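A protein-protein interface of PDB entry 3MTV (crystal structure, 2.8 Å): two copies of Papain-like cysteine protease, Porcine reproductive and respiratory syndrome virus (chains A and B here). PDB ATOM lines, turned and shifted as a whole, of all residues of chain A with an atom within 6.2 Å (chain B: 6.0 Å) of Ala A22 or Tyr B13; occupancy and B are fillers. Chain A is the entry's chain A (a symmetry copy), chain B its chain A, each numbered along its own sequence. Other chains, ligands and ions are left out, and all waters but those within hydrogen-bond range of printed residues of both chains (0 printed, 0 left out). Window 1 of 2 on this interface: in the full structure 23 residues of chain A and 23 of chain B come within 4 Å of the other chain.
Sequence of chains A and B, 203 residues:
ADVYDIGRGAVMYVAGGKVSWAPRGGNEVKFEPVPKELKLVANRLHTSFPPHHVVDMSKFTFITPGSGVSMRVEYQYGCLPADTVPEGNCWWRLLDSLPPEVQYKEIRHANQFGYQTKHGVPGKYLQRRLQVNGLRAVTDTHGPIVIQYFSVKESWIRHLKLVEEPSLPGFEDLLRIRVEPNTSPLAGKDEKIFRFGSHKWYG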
ATOM      1  N   ILE A   6     -23.391 -15.064  -7.911  1.00  0.00           N
ATOM      2  CA  ILE A   6     -21.951 -14.932  -7.865  1.00  0.00           C
ATOM      3  C   ILE A   6     -21.429 -14.462  -9.169  1.00  0.00           C
ATOM      4  O   ILE A   6     -20.212 -14.498  -9.421  1.00  0.00           O
ATOM      5  CB  ILE A   6     -21.262 -16.253  -7.623  1.00  0.00           C
ATOM      6  CG1 ILE A   6     -21.549 -17.195  -8.830  1.00  0.00           C
ATOM      7  CG2 ILE A   6     -21.677 -16.877  -6.314  1.00  0.00           C
ATOM      8  CD1 ILE A   6     -20.814 -18.600  -8.642  1.00  0.00           C
ATOM      9  N   GLY A   9     -23.658 -15.506 -14.557  1.00  0.00           N
ATOM     10  CA  GLY A   9     -24.600 -16.524 -14.969  1.00  0.00           C
ATOM     11  C   GLY A   9     -24.727 -17.680 -13.989  1.00  0.00           C
ATOM     12  O   GLY A   9     -25.580 -18.471 -14.136  1.00  0.00           O
ATOM     13  N   ALA A  10     -23.950 -17.734 -12.935  1.00  0.00           N
ATOM     14  CA  ALA A  10     -24.112 -18.768 -11.930  1.00  0.00           C
ATOM     15  C   ALA A  10     -24.620 -18.350 -10.544  1.00  0.00           C
ATOM     16  O   ALA A  10     -24.734 -17.107 -10.189  1.00  0.00           O
ATOM     17  CB  ALA A  10     -22.779 -19.350 -11.705  1.00  0.00           C
ATOM     18  N   VAL A  11     -24.772 -19.394  -9.713  1.00  0.00           N
ATOM     19  CA  VAL A  11     -25.051 -19.128  -8.333  1.00  0.00           C
ATOM     20  C   VAL A  11     -24.399 -20.191  -7.518  1.00  0.00           C
ATOM     21  O   VAL A  11     -24.019 -21.177  -8.066  1.00  0.00           O
ATOM     22  CB  VAL A  11     -26.559 -19.294  -8.040  1.00  0.00           C
ATOM     23  CG1 VAL A  11     -27.335 -18.212  -8.662  1.00  0.00           C
ATOM     24  CG2 VAL A  11     -27.090 -20.657  -8.488  1.00  0.00           C
ATOM     25  N   MET A  12     -24.342 -20.095  -6.197  1.00  0.00           N
ATOM     26  CA  MET A  12     -23.512 -21.085  -5.578  1.00  0.00           C
ATOM     27  C   MET A  12     -24.110 -21.507  -4.328  1.00  0.00           C
ATOM     28  O   MET A  12     -24.626 -20.656  -3.649  1.00  0.00           O
ATOM     29  CB  MET A  12     -22.187 -20.449  -5.209  1.00  0.00           C
ATOM     30  CG  MET A  12     -21.497 -21.188  -4.110  1.00  0.00           C
ATOM     31  SD  MET A  12     -19.794 -20.681  -3.751  1.00  0.00           S
ATOM     32  CE  MET A  12     -19.947 -19.107  -2.947  1.00  0.00           C
ATOM     33  N   TYR A  13     -24.067 -22.799  -4.007  1.00  0.00           N
ATOM     34  CA  TYR A  13     -24.792 -23.244  -2.853  1.00  0.00           C
ATOM     35  C   TYR A  13     -23.739 -23.569  -1.876  1.00  0.00           C
ATOM     36  O   TYR A  13     -22.705 -24.035  -2.295  1.00  0.00           O
ATOM     37  CB  TYR A  13     -25.540 -24.534  -3.092  1.00  0.00           C
ATOM     38  CG  TYR A  13     -26.568 -24.634  -4.208  1.00  0.00           C
ATOM     39  CD1 TYR A  13     -26.651 -23.708  -5.213  1.00  0.00           C
ATOM     40  CD2 TYR A  13     -27.454 -25.722  -4.259  1.00  0.00           C
ATOM     41  CE1 TYR A  13     -27.593 -23.866  -6.273  1.00  0.00           C
ATOM     42  CE2 TYR A  13     -28.415 -25.866  -5.313  1.00  0.00           C
ATOM     43  CZ  TYR A  13     -28.469 -24.939  -6.300  1.00  0.00           C
ATOM     44  OH  TYR A  13     -29.375 -25.056  -7.295  1.00  0.00           O
ATOM     45  N   SER A  20     -21.190 -25.777  -4.121  1.00  0.00           N
ATOM     46  CA  SER A  20     -21.597 -26.258  -5.427  1.00  0.00           C
ATOM     47  C   SER A  20     -21.885 -25.065  -6.297  1.00  0.00           C
ATOM     48  O   SER A  20     -22.243 -24.047  -5.831  1.00  0.00           O
ATOM     49  CB  SER A  20     -22.882 -27.096  -5.330  1.00  0.00           C
ATOM     50  OG  SER A  20     -23.721 -26.907  -6.501  1.00  0.00           O
ATOM     51  N   TRP A  21     -21.826 -25.162  -7.594  1.00  0.00           N
ATOM     52  CA  TRP A  21     -22.463 -24.050  -8.252  1.00  0.00           C
ATOM     53  C   TRP A  21     -23.433 -24.531  -9.307  1.00  0.00           C
ATOM     54  O   TRP A  21     -23.378 -25.646  -9.653  1.00  0.00           O
ATOM     55  CB  TRP A  21     -21.425 -23.175  -8.906  1.00  0.00           C
ATOM     56  CG  TRP A  21     -20.708 -23.757 -10.143  1.00  0.00           C
ATOM     57  CD1 TRP A  21     -19.656 -24.646 -10.128  1.00  0.00           C
ATOM     58  CD2 TRP A  21     -20.965 -23.497 -11.531  1.00  0.00           C
ATOM     59  NE1 TRP A  21     -19.234 -24.941 -11.419  1.00  0.00           N
ATOM     60  CE2 TRP A  21     -19.991 -24.233 -12.295  1.00  0.00           C
ATOM     61  CE3 TRP A  21     -21.896 -22.719 -12.207  1.00  0.00           C
ATOM     62  CZ2 TRP A  21     -19.939 -24.240 -13.684  1.00  0.00           C
ATOM     63  CZ3 TRP A  21     -21.828 -22.667 -13.641  1.00  0.00           C
ATOM     64  CH2 TRP A  21     -20.863 -23.456 -14.346  1.00  0.00           C
ATOM     65  N   ALA A  22     -24.218 -23.644  -9.897  1.00  0.00           N
ATOM     66  CA  ALA A  22     -25.212 -24.037 -10.864  1.00  0.00           C
ATOM     67  C   ALA A  22     -25.547 -22.826 -11.689  1.00  0.00           C
ATOM     68  O   ALA A  22     -25.298 -21.715 -11.230  1.00  0.00           O
ATOM     69  CB  ALA A  22     -26.411 -24.529 -10.133  1.00  0.00           C
ATOM     70  N   PRO A  23     -26.145 -23.007 -12.890  1.00  0.00           N
ATOM     71  CA  PRO A  23     -26.471 -21.795 -13.670  1.00  0.00           C
ATOM     72  C   PRO A  23     -27.660 -21.044 -13.038  1.00  0.00           C
ATOM     73  O   PRO A  23     -28.294 -21.649 -12.167  1.00  0.00           O
ATOM     74  CB  PRO A  23     -26.743 -22.306 -15.098  1.00  0.00           C
ATOM     75  CG  PRO A  23     -26.195 -23.625 -15.138  1.00  0.00           C
ATOM     76  CD  PRO A  23     -26.258 -24.214 -13.705  1.00  0.00           C
ATOM     77  N   ARG A  24     -27.906 -19.778 -13.421  1.00  0.00           N
ATOM     78  CA  ARG A  24     -28.643 -18.818 -12.600  1.00  0.00           C
ATOM     79  C   ARG A  24     -30.017 -19.296 -12.925  1.00  0.00           C
ATOM     80  O   ARG A  24     -30.783 -19.794 -12.039  1.00  0.00           O
ATOM     81  CB  ARG A  24     -28.389 -17.356 -13.055  1.00  0.00           C
ATOM     82  CG  ARG A  24     -29.274 -16.185 -12.504  1.00  0.00           C
ATOM     83  CD  ARG A  24     -28.680 -14.795 -13.041  1.00  0.00           C
ATOM     84  NE  ARG A  24     -29.671 -13.684 -13.185  1.00  0.00           N
ATOM     85  CZ  ARG A  24     -29.737 -12.488 -12.500  1.00  0.00           C
ATOM     86  NH1 ARG A  24     -28.824 -12.089 -11.511  1.00  0.00           N
ATOM     87  NH2 ARG A  24     -30.766 -11.643 -12.834  1.00  0.00           N
ATOM     88  N   PRO A  51     -20.646 -27.530 -13.015  1.00  0.00           N
ATOM     89  CA  PRO A  51     -21.847 -27.244 -12.251  1.00  0.00           C
ATOM     90  C   PRO A  51     -22.313 -28.490 -11.572  1.00  0.00           C
ATOM     91  O   PRO A  51     -22.066 -29.487 -12.081  1.00  0.00           O
ATOM     92  CB  PRO A  51     -22.799 -26.903 -13.313  1.00  0.00           C
ATOM     93  CG  PRO A  51     -22.097 -26.900 -14.650  1.00  0.00           C
ATOM     94  CD  PRO A  51     -20.972 -27.742 -14.425  1.00  0.00           C
ATOM     95  N   HIS A  52     -22.804 -28.440 -10.358  1.00  0.00           N
ATOM     96  CA  HIS A  52     -23.714 -29.455  -9.854  1.00  0.00           C
ATOM     97  C   HIS A  52     -22.890 -30.459  -9.258  1.00  0.00           C
ATOM     98  O   HIS A  52     -23.424 -31.470  -8.706  1.00  0.00           O
ATOM     99  CB  HIS A  52     -24.631 -30.124 -10.931  1.00  0.00           C
ATOM    100  CG  HIS A  52     -25.461 -29.168 -11.791  1.00  0.00           C
ATOM    101  ND1 HIS A  52     -26.398 -28.270 -11.278  1.00  0.00           N
ATOM    102  CD2 HIS A  52     -25.506 -29.006 -13.141  1.00  0.00           C
ATOM    103  CE1 HIS A  52     -26.944 -27.596 -12.285  1.00  0.00           C
ATOM    104  NE2 HIS A  52     -26.443 -28.046 -13.438  1.00  0.00           N
ATOM    105  N   HIS A  53     -21.579 -30.213  -9.300  1.00  0.00           N
ATOM    106  CA  HIS A  53     -20.817 -31.039  -8.374  1.00  0.00           C
ATOM    107  C   HIS A  53     -20.412 -30.321  -7.150  1.00  0.00           C
ATOM    108  O   HIS A  53     -20.045 -29.165  -7.227  1.00  0.00           O
ATOM    109  CB  HIS A  53     -19.598 -31.701  -8.955  1.00  0.00           C
ATOM    110  CG  HIS A  53     -19.833 -32.427 -10.240  1.00  0.00           C
ATOM    111  ND1 HIS A  53     -20.379 -31.824 -11.356  1.00  0.00           N
ATOM    112  CD2 HIS A  53     -19.563 -33.710 -10.588  1.00  0.00           C
ATOM    113  CE1 HIS A  53     -20.427 -32.705 -12.330  1.00  0.00           C
ATOM    114  NE2 HIS A  53     -19.930 -33.842 -11.890  1.00  0.00           N
ATOM    115  N   VAL A  54     -20.475 -31.067  -6.056  1.00  0.00           N
ATOM    116  CA  VAL A  54     -20.173 -30.659  -4.713  1.00  0.00           C
ATOM    117  C   VAL A  54     -18.720 -30.988  -4.333  1.00  0.00           C
ATOM    118  O   VAL A  54     -18.188 -32.088  -4.612  1.00  0.00           O
ATOM    119  CB  VAL A  54     -21.183 -31.419  -3.819  1.00  0.00           C
ATOM    120  CG1 VAL A  54     -20.575 -31.961  -2.630  1.00  0.00           C
ATOM    121  CG2 VAL A  54     -22.413 -30.472  -3.484  1.00  0.00           C
ATOM    122  N   ASP B   2     -27.197 -36.431  -4.211  1.00  0.00           N
ATOM    123  CA  ASP B   2     -27.385 -37.253  -5.507  1.00  0.00           C
ATOM    124  C   ASP B   2     -28.019 -36.477  -6.690  1.00  0.00           C
ATOM    125  O   ASP B   2     -28.818 -35.622  -6.446  1.00  0.00           O
ATOM    126  CB  ASP B   2     -28.423 -38.338  -5.345  1.00  0.00           C
ATOM    127  CG  ASP B   2     -27.844 -39.763  -5.398  1.00  0.00           C
ATOM    128  OD1 ASP B   2     -27.454 -40.317  -6.486  1.00  0.00           O
ATOM    129  OD2 ASP B   2     -27.833 -40.370  -4.302  1.00  0.00           O
ATOM    130  N   VAL B   3     -27.824 -36.793  -7.960  1.00  0.00           N
ATOM    131  CA  VAL B   3     -28.252 -35.780  -8.981  1.00  0.00           C
ATOM    132  C   VAL B   3     -28.640 -36.290 -10.369  1.00  0.00           C
ATOM    133  O   VAL B   3     -27.881 -37.016 -10.968  1.00  0.00           O
ATOM    134  CB  VAL B   3     -27.122 -34.741  -9.201  1.00  0.00           C
ATOM    135  CG1 VAL B   3     -27.381 -33.721 -10.333  1.00  0.00           C
ATOM    136  CG2 VAL B   3     -26.939 -34.026  -8.010  1.00  0.00           C
ATOM    137  N   TYR B   4     -29.785 -35.906 -10.945  1.00  0.00           N
ATOM    138  CA  TYR B   4     -30.278 -36.606 -12.152  1.00  0.00           C
ATOM    139  C   TYR B   4     -30.740 -35.640 -13.179  1.00  0.00           C
ATOM    140  O   TYR B   4     -31.276 -34.642 -12.801  1.00  0.00           O
ATOM    141  CB  TYR B   4     -31.489 -37.427 -11.772  1.00  0.00           C
ATOM    142  CG  TYR B   4     -31.258 -38.418 -10.640  1.00  0.00           C
ATOM    143  CD1 TYR B   4     -31.522 -38.075  -9.305  1.00  0.00           C
ATOM    144  CD2 TYR B   4     -30.770 -39.702 -10.886  1.00  0.00           C
ATOM    145  CE1 TYR B   4     -31.311 -38.980  -8.254  1.00  0.00           C
ATOM    146  CE2 TYR B   4     -30.540 -40.614  -9.814  1.00  0.00           C
ATOM    147  CZ  TYR B   4     -30.845 -40.268  -8.525  1.00  0.00           C
ATOM    148  OH  TYR B   4     -30.616 -41.183  -7.495  1.00  0.00           O
ATOM    149  N   VAL B  11     -32.129 -30.242 -13.897  1.00  0.00           N
ATOM    150  CA  VAL B  11     -31.651 -31.426 -13.247  1.00  0.00           C
ATOM    151  C   VAL B  11     -32.083 -31.376 -11.823  1.00  0.00           C
ATOM    152  O   VAL B  11     -32.473 -30.342 -11.381  1.00  0.00           O
ATOM    153  CB  VAL B  11     -30.107 -31.423 -13.179  1.00  0.00           C
ATOM    154  CG1 VAL B  11     -29.523 -31.621 -14.513  1.00  0.00           C
ATOM    155  CG2 VAL B  11     -29.557 -30.147 -12.539  1.00  0.00           C
ATOM    156  N   MET B  12     -31.931 -32.428 -11.030  1.00  0.00           N
ATOM    157  CA  MET B  12     -32.575 -32.294  -9.758  1.00  0.00           C
ATOM    158  C   MET B  12     -31.754 -32.902  -8.732  1.00  0.00           C
ATOM    159  O   MET B  12     -31.198 -33.934  -9.010  1.00  0.00           O
ATOM    160  CB  MET B  12     -33.866 -33.088  -9.778  1.00  0.00           C
ATOM    161  CG  MET B  12     -34.313 -33.468  -8.405  1.00  0.00           C
ATOM    162  SD  MET B  12     -35.968 -34.195  -8.274  1.00  0.00           S
ATOM    163  CE  MET B  12     -35.802 -35.827  -8.952  1.00  0.00           C
ATOM    164  N   TYR B  13     -31.649 -32.288  -7.554  1.00  0.00           N
ATOM    165  CA  TYR B  13     -30.716 -32.800  -6.594  1.00  0.00           C
ATOM    166  C   TYR B  13     -31.570 -33.389  -5.549  1.00  0.00           C
ATOM    167  O   TYR B  13     -32.621 -32.844  -5.305  1.00  0.00           O
ATOM    168  CB  TYR B  13     -29.924 -31.712  -5.909  1.00  0.00           C
ATOM    169  CG  TYR B  13     -29.086 -30.738  -6.723  1.00  0.00           C
ATOM    170  CD1 TYR B  13     -29.234 -30.598  -8.076  1.00  0.00           C
ATOM    171  CD2 TYR B  13     -28.142 -29.914  -6.088  1.00  0.00           C
ATOM    172  CE1 TYR B  13     -28.469 -29.634  -8.797  1.00  0.00           C
ATOM    173  CE2 TYR B  13     -27.357 -28.964  -6.818  1.00  0.00           C
ATOM    174  CZ  TYR B  13     -27.532 -28.838  -8.157  1.00  0.00           C
ATOM    175  OH  TYR B  13     -26.792 -27.952  -8.860  1.00  0.00           O
ATOM    176  N   VAL B  14     -31.087 -34.453  -4.882  1.00  0.00           N
ATOM    177  CA  VAL B  14     -31.807 -35.169  -3.827  1.00  0.00           C
ATOM    178  C   VAL B  14     -31.009 -35.720  -2.664  1.00  0.00           C
ATOM    179  O   VAL B  14     -29.945 -36.309  -2.911  1.00  0.00           O
ATOM    180  CB  VAL B  14     -32.240 -36.421  -4.385  1.00  0.00           C
ATOM    181  CG1 VAL B  14     -33.054 -37.090  -3.376  1.00  0.00           C
ATOM    182  CG2 VAL B  14     -33.022 -36.232  -5.713  1.00  0.00           C
ATOM    183  N   ALA B  15     -31.540 -35.644  -1.438  1.00  0.00           N
ATOM    184  CA  ALA B  15     -30.734 -35.799  -0.226  1.00  0.00           C
ATOM    185  C   ALA B  15     -31.605 -35.526   0.969  1.00  0.00           C
ATOM    186  O   ALA B  15     -32.069 -34.427   1.109  1.00  0.00           O
ATOM    187  CB  ALA B  15     -29.610 -34.770  -0.261  1.00  0.00           C
ATOM    188  N   LYS B  18     -35.552 -34.355   1.046  1.00  0.00           N
ATOM    189  CA  LYS B  18     -35.401 -33.001   0.503  1.00  0.00           C
ATOM    190  C   LYS B  18     -34.808 -32.991  -0.921  1.00  0.00           C
ATOM    191  O   LYS B  18     -33.969 -33.782  -1.261  1.00  0.00           O
ATOM    192  CB  LYS B  18     -34.591 -32.120   1.480  1.00  0.00           C
ATOM    193  CG  LYS B  18     -35.267 -31.794   2.844  1.00  0.00           C
ATOM    194  CD  LYS B  18     -34.444 -30.876   3.798  1.00  0.00           C
ATOM    195  CE  LYS B  18     -35.170 -30.669   5.190  1.00  0.00           C
ATOM    196  NZ  LYS B  18     -35.001 -29.306   5.877  1.00  0.00           N
ATOM    197  N   VAL B  19     -35.211 -32.022  -1.724  1.00  0.00           N
ATOM    198  CA  VAL B  19     -35.040 -32.051  -3.167  1.00  0.00           C
ATOM    199  C   VAL B  19     -34.985 -30.616  -3.823  1.00  0.00           C
ATOM    200  O   VAL B  19     -35.504 -29.647  -3.264  1.00  0.00           O
ATOM    201  CB  VAL B  19     -36.192 -32.809  -3.593  1.00  0.00           C
ATOM    202  CG1 VAL B  19     -36.733 -32.341  -4.900  1.00  0.00           C
ATOM    203  CG2 VAL B  19     -35.838 -34.283  -3.492  1.00  0.00           C
ATOM    204  N   SER B  20     -34.280 -30.440  -4.943  1.00  0.00           N
ATOM    205  CA  SER B  20     -34.056 -29.118  -5.495  1.00  0.00           C
ATOM    206  C   SER B  20     -34.001 -29.239  -6.994  1.00  0.00           C
ATOM    207  O   SER B  20     -33.648 -30.235  -7.508  1.00  0.00           O
ATOM    208  CB  SER B  20     -32.714 -28.541  -5.016  1.00  0.00           C
ATOM    209  OG  SER B  20     -32.092 -27.732  -6.051  1.00  0.00           O
ATOM    210  N   TRP B  21     -34.262 -28.213  -7.751  1.00  0.00           N
ATOM    211  CA  TRP B  21     -33.823 -28.414  -9.109  1.00  0.00           C
ATOM    212  C   TRP B  21     -33.004 -27.237  -9.590  1.00  0.00           C
ATOM    213  O   TRP B  21     -33.033 -26.244  -8.974  1.00  0.00           O
ATOM    214  CB  TRP B  21     -35.015 -28.582 -10.015  1.00  0.00           C
ATOM    215  CG  TRP B  21     -35.878 -27.327 -10.265  1.00  0.00           C
ATOM    216  CD1 TRP B  21     -36.846 -26.826  -9.423  1.00  0.00           C
ATOM    217  CD2 TRP B  21     -35.869 -26.446 -11.399  1.00  0.00           C
ATOM    218  NE1 TRP B  21     -37.449 -25.699  -9.970  1.00  0.00           N
ATOM    219  CE2 TRP B  21     -36.897 -25.460 -11.187  1.00  0.00           C
ATOM    220  CE3 TRP B  21     -35.120 -26.390 -12.566  1.00  0.00           C
ATOM    221  CZ2 TRP B  21     -37.173 -24.425 -12.072  1.00  0.00           C
ATOM    222  CZ3 TRP B  21     -35.423 -25.361 -13.522  1.00  0.00           C
ATOM    223  CH2 TRP B  21     -36.429 -24.383 -13.234  1.00  0.00           C
ATOM    224  N   ALA B  22     -32.393 -27.328 -10.759  1.00  0.00           N
ATOM    225  CA  ALA B  22     -31.542 -26.274 -11.253  1.00  0.00           C
ATOM    226  C   ALA B  22     -31.436 -26.437 -12.744  1.00  0.00           C
ATOM    227  O   ALA B  22     -31.687 -27.534 -13.234  1.00  0.00           O
ATOM    228  CB  ALA B  22     -30.208 -26.404 -10.608  1.00  0.00           C
ATOM    229  N   PRO B  23     -31.028 -25.379 -13.482  1.00  0.00           N
ATOM    230  CA  PRO B  23     -30.923 -25.577 -14.943  1.00  0.00           C
ATOM    231  C   PRO B  23     -29.705 -26.458 -15.286  1.00  0.00           C
ATOM    232  O   PRO B  23     -28.896 -26.660 -14.375  1.00  0.00           O
ATOM    233  CB  PRO B  23     -30.849 -24.154 -15.531  1.00  0.00           C
ATOM    234  CG  PRO B  23     -31.298 -23.290 -14.484  1.00  0.00           C
ATOM    235  CD  PRO B  23     -30.961 -23.963 -13.129  1.00  0.00           C
ATOM    236  N   LEU B  45     -42.073 -30.891  -8.458  1.00  0.00           N
ATOM    237  CA  LEU B  45     -40.892 -30.006  -8.421  1.00  0.00           C
ATOM    238  C   LEU B  45     -40.643 -29.062  -9.538  1.00  0.00           C
ATOM    239  O   LEU B  45     -40.650 -27.909  -9.358  1.00  0.00           O
ATOM    240  CB  LEU B  45     -39.616 -30.793  -8.417  1.00  0.00           C
ATOM    241  CG  LEU B  45     -38.669 -30.183  -7.382  1.00  0.00           C
ATOM    242  CD1 LEU B  45     -37.294 -30.429  -7.754  1.00  0.00           C
ATOM    243  CD2 LEU B  45     -38.881 -28.725  -7.298  1.00  0.00           C
ATOM    244  N   HIS B  52     -33.508 -23.909  -7.255  1.00  0.00           N
ATOM    245  CA  HIS B  52     -32.456 -23.545  -6.320  1.00  0.00           C
ATOM    246  C   HIS B  52     -33.097 -23.384  -5.053  1.00  0.00           C
ATOM    247  O   HIS B  52     -32.408 -23.086  -4.028  1.00  0.00           O
ATOM    248  CB  HIS B  52     -31.678 -22.231  -6.667  1.00  0.00           C
ATOM    249  CG  HIS B  52     -31.072 -22.164  -8.070  1.00  0.00           C
ATOM    250  ND1 HIS B  52     -30.133 -23.073  -8.559  1.00  0.00           N
ATOM    251  CD2 HIS B  52     -31.258 -21.261  -9.071  1.00  0.00           C
ATOM    252  CE1 HIS B  52     -29.808 -22.729  -9.801  1.00  0.00           C
ATOM    253  NE2 HIS B  52     -30.455 -21.609 -10.130  1.00  0.00           N
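Of the 16 printed residues of chain B, 5 touch a printed residue of chain A. Hydrophobic or aromatic side chains of chain A within 4 Å of the printed part of chain B: Val A11, Tyr A13, Ala A22, Pro A23 and His A52. Among the printed residues, no Asp or Glu carboxylate lies within 4 Å of a Lys or Arg side-chain nitrogen of the other chain.
Val A11 touches His B52 (CG2 to CE1, 3.7 Å). Tyr B13 touches Tyr A13 (CE2 to CE2, 3.6 Å). Tyr A13 touches Ala B22 (OH to CB, 3.7 Å). Ala A22 touches Tyr B13 (CB to OH, 3.7 Å). Ala A22 touches His B52. Pro B23 touches Pro A23 (O to CD, 3.7 Å). His A52 touches Val B11. His A52 touches Ala B22 (CE1 to CB, 3.9 Å).
The backbone NH (N) of Val B11 lies within hydrogen-bond range of the backbone carbonyl oxygen (O) of Ala B22, at 2.8 Å. The backbone carbonyl oxygen (O) of Ser B20 lies within hydrogen-bond range of the backbone NH (N) of Tyr B13, at 2.9 Å. O of Trp B21 lies within hydrogen-bond range of N of His B52 (2.9 Å). O of Gly A9 lies within hydrogen-bond range of N of Arg A24, at 2.8 Å. The backbone NH (N) of Val A11 sits at hydrogen-bond distance from the backbone carbonyl oxygen (O) of Ala A22, 2.8 Å away. The backbone NH of Tyr A13 is in hydrogen-bond range of the backbone carbonyl oxygen of Ser A20.
Of the printed residues of chain B, Val A11 touches His B52. Of the printed residues of chain B, Tyr A13 touches Tyr B13 (3.6 Å), Ala B22 (3.7 Å) and His B52 (2.5 Å). Ala A22 touches just these residues of chain B: Tyr B13 (3.7 Å) and His B52 (3.9 Å). Of the printed residues of chain A, Tyr B13 touches Tyr A13 (3.6 Å), Ala A22 (3.7 Å) and His A52 (2.5 Å).
Val A11 touches His B52, and with the chains exchanged His A52 touches Val B11. Tyr B13 touches its own counterpart, Tyr A13. Tyr A13 touches Ala B22, and with the chains exchanged Ala A22 touches Tyr B13. Tyr A13 touches His B52, and with the chains exchanged His A52 touches Tyr B13. 8 positions are printed for both chains. Of the 13 pairs that touch across the chains among the printed residues, 12 have their exchanged pair printed and touching as well.
The side-chain hydroxyl (OH) of Tyr B13 is in hydrogen-bond range of a ring nitrogen (ND1) of His A52 (2.5 Å). NE2 of His A52 is in hydrogen-bond range of O of Pro B23. ND1 of His B52 lies within hydrogen-bond range of OH of Tyr A13 (2.5 Å). The backbone carbonyl oxygen of Pro A23 lies within hydrogen-bond range of a ring nitrogen (NE2) of His B52. The backbone carbonyl oxygen (O) of Arg A24 lies within hydrogen-bond range of a ring nitrogen (NE2) of His B52, at 2.7 Å.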
